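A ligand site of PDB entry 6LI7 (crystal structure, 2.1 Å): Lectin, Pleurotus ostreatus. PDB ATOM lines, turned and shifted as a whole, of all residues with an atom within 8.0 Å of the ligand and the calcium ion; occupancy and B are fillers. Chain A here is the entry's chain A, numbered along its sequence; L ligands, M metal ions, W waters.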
ATOM      1  N   TRP A 222      30.376  -6.250   8.744  1.00  0.00           N
ATOM      2  CA  TRP A 222      31.058  -7.554   8.848  1.00  0.00           C
ATOM      3  C   TRP A 222      32.579  -7.307   8.782  1.00  0.00           C
ATOM      4  O   TRP A 222      33.049  -6.138   8.630  1.00  0.00           O
ATOM      5  CB  TRP A 222      30.538  -8.489   7.728  1.00  0.00           C
ATOM      6  CG  TRP A 222      30.614  -9.952   8.023  1.00  0.00           C
ATOM      7  CD1 TRP A 222      31.468 -10.828   7.438  1.00  0.00           C
ATOM      8  CD2 TRP A 222      29.848 -10.702   8.974  1.00  0.00           C
ATOM      9  NE1 TRP A 222      31.274 -12.064   7.948  1.00  0.00           N
ATOM     10  CE2 TRP A 222      30.291 -12.030   8.907  1.00  0.00           C
ATOM     11  CE3 TRP A 222      28.821 -10.399   9.878  1.00  0.00           C
ATOM     12  CZ2 TRP A 222      29.759 -13.052   9.684  1.00  0.00           C
ATOM     13  CZ3 TRP A 222      28.304 -11.409  10.666  1.00  0.00           C
ATOM     14  CH2 TRP A 222      28.747 -12.728  10.547  1.00  0.00           C
ATOM     15  N   GLY A 229      28.443  -9.761  -2.123  1.00  0.00           N
ATOM     16  CA  GLY A 229      27.119 -10.135  -1.580  1.00  0.00           C
ATOM     17  C   GLY A 229      27.124 -11.434  -0.789  1.00  0.00           C
ATOM     18  O   GLY A 229      26.043 -11.983  -0.518  1.00  0.00           O
ATOM     19  N   ALA A 230      28.291 -11.944  -0.429  1.00  0.00           N
ATOM     20  CA  ALA A 230      28.377 -13.182   0.368  1.00  0.00           C
ATOM     21  C   ALA A 230      29.639 -13.108   1.219  1.00  0.00           C
ATOM     22  O   ALA A 230      30.555 -12.291   0.930  1.00  0.00           O
ATOM     23  CB  ALA A 230      28.353 -14.402  -0.517  1.00  0.00           C
ATOM     24  N   ALA A 231      29.660 -13.889   2.278  1.00  0.00           N
ATOM     25  CA  ALA A 231      30.877 -13.988   3.118  1.00  0.00           C
ATOM     26  C   ALA A 231      31.069 -15.445   3.404  1.00  0.00           C
ATOM     27  O   ALA A 231      30.092 -16.184   3.346  1.00  0.00           O
ATOM     28  CB  ALA A 231      30.692 -13.240   4.412  1.00  0.00           C
ATOM     29  N   PRO A 232      32.279 -15.847   3.839  1.00  0.00           N
ATOM     30  CA  PRO A 232      32.532 -17.240   4.179  1.00  0.00           C
ATOM     31  C   PRO A 232      31.656 -17.696   5.336  1.00  0.00           C
ATOM     32  O   PRO A 232      31.165 -16.868   6.129  1.00  0.00           O
ATOM     33  CB  PRO A 232      34.034 -17.279   4.529  1.00  0.00           C
ATOM     34  CG  PRO A 232      34.604 -16.038   3.889  1.00  0.00           C
ATOM     35  CD  PRO A 232      33.492 -15.010   3.877  1.00  0.00           C
ATOM     36  N   VAL A 233      31.432 -19.015   5.378  1.00  0.00           N
ATOM     37  CA  VAL A 233      30.810 -19.690   6.543  1.00  0.00           C
ATOM     38  C   VAL A 233      31.789 -19.499   7.709  1.00  0.00           C
ATOM     39  O   VAL A 233      32.979 -19.548   7.469  1.00  0.00           O
ATOM     40  CB  VAL A 233      30.516 -21.167   6.266  1.00  0.00           C
ATOM     41  CG1 VAL A 233      29.976 -21.854   7.512  1.00  0.00           C
ATOM     42  CG2 VAL A 233      29.529 -21.325   5.103  1.00  0.00           C
ATOM     43  N   ALA A 258      21.302 -10.300  13.513  1.00  0.00           N
ATOM     44  CA  ALA A 258      22.422 -10.766  12.686  1.00  0.00           C
ATOM     45  C   ALA A 258      21.965 -11.797  11.647  1.00  0.00           C
ATOM     46  O   ALA A 258      21.164 -12.671  11.959  1.00  0.00           O
ATOM     47  CB  ALA A 258      23.501 -11.337  13.587  1.00  0.00           C
ATOM     48  N   ASP A 259      22.612 -11.752  10.490  1.00  0.00           N
ATOM     49  CA  ASP A 259      22.583 -12.810   9.472  1.00  0.00           C
ATOM     50  C   ASP A 259      23.837 -13.706   9.606  1.00  0.00           C
ATOM     51  O   ASP A 259      24.893 -13.181   9.261  1.00  0.00           O
ATOM     52  CB  ASP A 259      22.519 -12.211   8.084  1.00  0.00           C
ATOM     53  CG  ASP A 259      22.478 -13.254   6.979  1.00  0.00           C
ATOM     54  OD1 ASP A 259      22.739 -14.442   7.265  1.00  0.00           O
ATOM     55  OD2 ASP A 259      22.129 -12.867   5.857  1.00  0.00           O
ATOM     56  N   ASP A 260      23.744 -14.658  10.514  1.00  0.00           N
ATOM     57  CA  ASP A 260      22.702 -15.703  10.650  1.00  0.00           C
ATOM     58  C   ASP A 260      22.328 -15.708  12.126  1.00  0.00           C
ATOM     59  O   ASP A 260      21.160 -15.956  12.452  1.00  0.00           O
ATOM     60  CB  ASP A 260      23.125 -17.072  10.110  1.00  0.00           C
ATOM     61  CG  ASP A 260      22.816 -17.206   8.640  1.00  0.00           C
ATOM     62  OD1 ASP A 260      21.602 -17.237   8.330  1.00  0.00           O
ATOM     63  OD2 ASP A 260      23.767 -17.152   7.803  1.00  0.00           O
ATOM     64  N   ARG A 261      23.275 -15.364  13.021  1.00  0.00           N
ATOM     65  CA  ARG A 261      23.077 -15.534  14.479  1.00  0.00           C
ATOM     66  C   ARG A 261      24.157 -14.734  15.231  1.00  0.00           C
ATOM     67  O   ARG A 261      25.123 -14.301  14.593  1.00  0.00           O
ATOM     68  CB  ARG A 261      23.115 -17.023  14.842  1.00  0.00           C
ATOM     69  CG  ARG A 261      24.484 -17.675  14.679  1.00  0.00           C
ATOM     70  CD  ARG A 261      24.546 -19.207  14.723  1.00  0.00           C
ATOM     71  NE  ARG A 261      23.504 -19.744  15.570  1.00  0.00           N
ATOM     72  CZ  ARG A 261      22.434 -20.423  15.130  1.00  0.00           C
ATOM     73  NH1 ARG A 261      22.296 -20.690  13.842  1.00  0.00           N
ATOM     74  NH2 ARG A 261      21.498 -20.808  15.995  1.00  0.00           N
ATOM     75  N   TYR A 277      17.534 -12.738  11.214  1.00  0.00           N
ATOM     76  CA  TYR A 277      17.825 -11.491  10.504  1.00  0.00           C
ATOM     77  C   TYR A 277      16.510 -10.831  10.097  1.00  0.00           C
ATOM     78  O   TYR A 277      16.605  -9.797   9.466  1.00  0.00           O
ATOM     79  CB  TYR A 277      18.783 -11.738   9.358  1.00  0.00           C
ATOM     80  CG  TYR A 277      18.398 -12.818   8.373  1.00  0.00           C
ATOM     81  CD1 TYR A 277      17.580 -12.525   7.304  1.00  0.00           C
ATOM     82  CD2 TYR A 277      18.950 -14.082   8.464  1.00  0.00           C
ATOM     83  CE1 TYR A 277      17.251 -13.495   6.375  1.00  0.00           C
ATOM     84  CE2 TYR A 277      18.629 -15.067   7.550  1.00  0.00           C
ATOM     85  CZ  TYR A 277      17.771 -14.768   6.502  1.00  0.00           C
ATOM     86  OH  TYR A 277      17.452 -15.697   5.568  1.00  0.00           O
ATOM     87  N   THR A 300      27.775 -15.274  13.560  1.00  0.00           N
ATOM     88  CA  THR A 300      28.114 -16.462  12.745  1.00  0.00           C
ATOM     89  C   THR A 300      27.332 -16.413  11.424  1.00  0.00           C
ATOM     90  O   THR A 300      26.121 -16.241  11.474  1.00  0.00           O
ATOM     91  CB  THR A 300      27.834 -17.728  13.574  1.00  0.00           C
ATOM     92  OG1 THR A 300      28.576 -17.697  14.800  1.00  0.00           O
ATOM     93  CG2 THR A 300      28.166 -18.989  12.811  1.00  0.00           C
ATOM     94  N   ASN A 301      28.031 -16.590  10.306  1.00  0.00           N
ATOM     95  CA  ASN A 301      27.452 -16.824   8.961  1.00  0.00           C
ATOM     96  C   ASN A 301      27.349 -18.342   8.690  1.00  0.00           C
ATOM     97  O   ASN A 301      28.361 -19.058   8.701  1.00  0.00           O
ATOM     98  CB  ASN A 301      28.233 -16.093   7.872  1.00  0.00           C
ATOM     99  CG  ASN A 301      27.504 -16.199   6.526  1.00  0.00           C
ATOM    100  OD1 ASN A 301      26.296 -16.408   6.538  1.00  0.00           O
ATOM    101  ND2 ASN A 301      28.222 -16.124   5.411  1.00  0.00           N
ATOM    102  N   GLY A 302      26.127 -18.815   8.484  1.00  0.00           N
ATOM    103  CA  GLY A 302      25.793 -20.186   8.077  1.00  0.00           C
ATOM    104  C   GLY A 302      25.947 -20.393   6.570  1.00  0.00           C
ATOM    105  O   GLY A 302      25.839 -21.532   6.129  1.00  0.00           O
ATOM    106  N   GLY A 303      26.150 -19.320   5.810  1.00  0.00           N
ATOM    107  CA  GLY A 303      26.167 -19.369   4.341  1.00  0.00           C
ATOM    108  C   GLY A 303      25.561 -18.123   3.724  1.00  0.00           C
ATOM    109  O   GLY A 303      24.636 -17.551   4.314  1.00  0.00           O
ATOM    110  N   GLY A 304      26.068 -17.756   2.556  1.00  0.00           N
ATOM    111  CA  GLY A 304      25.619 -16.633   1.734  1.00  0.00           C
ATOM    112  C   GLY A 304      25.933 -15.313   2.415  1.00  0.00           C
ATOM    113  O   GLY A 304      27.000 -15.172   3.028  1.00  0.00           O
ATOM    114  N   PRO A 305      25.027 -14.321   2.234  1.00  0.00           N
ATOM    115  CA  PRO A 305      25.212 -12.981   2.791  1.00  0.00           C
ATOM    116  C   PRO A 305      25.380 -13.106   4.318  1.00  0.00           C
ATOM    117  O   PRO A 305      24.912 -14.132   4.953  1.00  0.00           O
ATOM    118  CB  PRO A 305      23.915 -12.204   2.420  1.00  0.00           C
ATOM    119  CG  PRO A 305      23.371 -12.949   1.180  1.00  0.00           C
ATOM    120  CD  PRO A 305      23.773 -14.397   1.437  1.00  0.00           C
ATOM    121  N   ALA A 306      25.995 -12.081   4.894  1.00  0.00           N
ATOM    122  CA  ALA A 306      26.206 -11.997   6.352  1.00  0.00           C
ATOM    123  C   ALA A 306      26.244 -10.532   6.775  1.00  0.00           C
ATOM    124  O   ALA A 306      26.713  -9.672   5.982  1.00  0.00           O
ATOM    125  CB  ALA A 306      27.488 -12.712   6.720  1.00  0.00           C
ATOM    126  N   GLY A 307      25.863 -10.297   8.022  1.00  0.00           N
ATOM    127  CA  GLY A 307      25.942  -8.943   8.597  1.00  0.00           C
ATOM    128  C   GLY A 307      25.437  -8.936  10.012  1.00  0.00           C
ATOM    129  O   GLY A 307      24.648  -9.825  10.413  1.00  0.00           O
ATOM    130  N   ALA A 362      19.210  -4.283   0.347  1.00  0.00           N
ATOM    131  CA  ALA A 362      19.147  -5.715  -0.035  1.00  0.00           C
ATOM    132  C   ALA A 362      20.366  -6.440   0.549  1.00  0.00           C
ATOM    133  O   ALA A 362      21.455  -5.899   0.602  1.00  0.00           O
ATOM    134  CB  ALA A 362      19.193  -5.842  -1.546  1.00  0.00           C
ATOM    135  N   PRO A 363      20.283  -7.710   0.882  1.00  0.00           N
ATOM    136  CA  PRO A 363      19.066  -8.482   0.707  1.00  0.00           C
ATOM    137  C   PRO A 363      18.055  -8.376   1.845  1.00  0.00           C
ATOM    138  O   PRO A 363      17.014  -8.927   1.742  1.00  0.00           O
ATOM    139  CB  PRO A 363      19.606  -9.937   0.703  1.00  0.00           C
ATOM    140  CG  PRO A 363      20.794  -9.835   1.638  1.00  0.00           C
ATOM    141  CD  PRO A 363      21.440  -8.514   1.280  1.00  0.00           C
ATOM    142  N   TRP A 364      18.430  -7.777   2.971  1.00  0.00           N
ATOM    143  CA  TRP A 364      17.577  -7.880   4.178  1.00  0.00           C
ATOM    144  C   TRP A 364      16.424  -6.862   4.055  1.00  0.00           C
ATOM    145  O   TRP A 364      15.428  -7.137   4.598  1.00  0.00           O
ATOM    146  CB  TRP A 364      18.404  -7.653   5.450  1.00  0.00           C
ATOM    147  CG  TRP A 364      19.648  -8.511   5.451  1.00  0.00           C
ATOM    148  CD1 TRP A 364      19.711  -9.850   5.701  1.00  0.00           C
ATOM    149  CD2 TRP A 364      20.979  -8.094   5.161  1.00  0.00           C
ATOM    150  NE1 TRP A 364      21.012 -10.272   5.599  1.00  0.00           N
ATOM    151  CE2 TRP A 364      21.803  -9.227   5.276  1.00  0.00           C
ATOM    152  CE3 TRP A 364      21.568  -6.863   4.858  1.00  0.00           C
ATOM    153  CZ2 TRP A 364      23.184  -9.168   5.057  1.00  0.00           C
ATOM    154  CZ3 TRP A 364      22.937  -6.806   4.658  1.00  0.00           C
ATOM    155  CH2 TRP A 364      23.741  -7.943   4.759  1.00  0.00           C
ATOM    156  N   GLY A 365      16.579  -5.716   3.437  1.00  0.00           N
ATOM    157  CA  GLY A 365      15.433  -4.787   3.321  1.00  0.00           C
ATOM    158  C   GLY A 365      15.174  -3.993   4.592  1.00  0.00           C
ATOM    159  O   GLY A 365      15.955  -4.098   5.560  1.00  0.00           O
HETATM  160  C1  LIG L   1      20.136 -17.106   2.493  1.00  0.00           C
HETATM  161  C2  LIG L   1      21.226 -17.613   3.469  1.00  0.00           C
HETATM  162  C3  LIG L   1      20.943 -16.990   4.858  1.00  0.00           C
HETATM  163  C4  LIG L   1      20.825 -15.476   4.660  1.00  0.00           C
HETATM  164  C5  LIG L   1      19.939 -15.048   3.450  1.00  0.00           C
HETATM  165  C6  LIG L   1      19.923 -13.539   3.315  1.00  0.00           C
HETATM  166  C7  LIG L   1      22.322 -19.746   2.847  1.00  0.00           C
HETATM  167  C8  LIG L   1      22.283 -21.235   3.039  1.00  0.00           C
HETATM  168  N1  LIG L   1      21.334 -19.096   3.463  1.00  0.00           N
HETATM  169  O1  LIG L   1      20.205 -17.735   1.268  1.00  0.00           O
HETATM  170  O2  LIG L   1      22.011 -17.234   5.836  1.00  0.00           O
HETATM  171  O3  LIG L   1      22.209 -14.972   4.480  1.00  0.00           O
HETATM  172  O4  LIG L   1      20.436 -15.705   2.246  1.00  0.00           O
HETATM  173  O5  LIG L   1      19.090 -13.095   2.300  1.00  0.00           O
HETATM  174  O6  LIG L   1      23.229 -19.224   2.140  1.00  0.00           O
HETATM  175 CA    CA M   1      23.945 -15.905   5.890  1.00  0.00          CA
HETATM  176  O   HOH W   1      22.584 -20.197   6.467  1.00  0.00           O
HETATM  177  O   HOH W   2      19.897 -16.463  -1.134  1.00  0.00           O
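O6 of the ligand sits at hydrogen-bond distance from N of Gly 304, 3.2 Å away.
The side-chain carboxylate of Asp 260 lies close to the backbone NH of Gly 302, 3.0 Å away.
O of Thr 300 sits at hydrogen-bond distance from N of Asp 260 (3.0 Å).
The side-chain carboxylate (OD2) of Asp 259 lies within hydrogen-bond range of the indole nitrogen (NE1) of Trp 364 (2.8 Å).
N of Asp 259 is in hydrogen-bond range of O of Gly 307.
O of Gly 304 lies within hydrogen-bond range of ND2 of Asn 301 (2.8 Å).
The side-chain amide nitrogen of Asn 301 is in hydrogen-bond range of the backbone carbonyl oxygen of Ala 231 (2.8 Å).
ND2 of Asn 301 is in hydrogen-bond range of O of Pro 232 (3.1 Å).
O of Gly 304 sits at hydrogen-bond distance from N of Ala 231 (3.0 Å).
Tyr 277 touches the ligand.
CB of Pro 363 touches O5 of the ligand, at 3.6 Å.
Seven residues have an atom within 4 Å of the ligand: Asp 259, Asp 260, Tyr 277, Gly 303, Gly 304, Pro 305 and Pro 363.
The nearest printed residue that does not touch the ligand is Trp 364 (4.1 Å).
O of Pro 305 binds the calcium ion, 2.2 Å away.
The side-chain carboxylate (OD2) of Asp 260 binds the calcium ion (2.3 Å).
The side-chain carboxylate (OD1) of Asp 259 is bound to the calcium ion, at 2.3 Å.
O2 of the ligand binds the calcium ion, at 2.3 Å.
The calcium ion is bound by O of Gly 303 (2.4 Å).
An oxygen (O3) of the ligand is bound to the calcium ion (2.4 Å).
The calcium ion is bound by the side-chain amide oxygen (OD1) of Asn 301 (2.5 Å).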
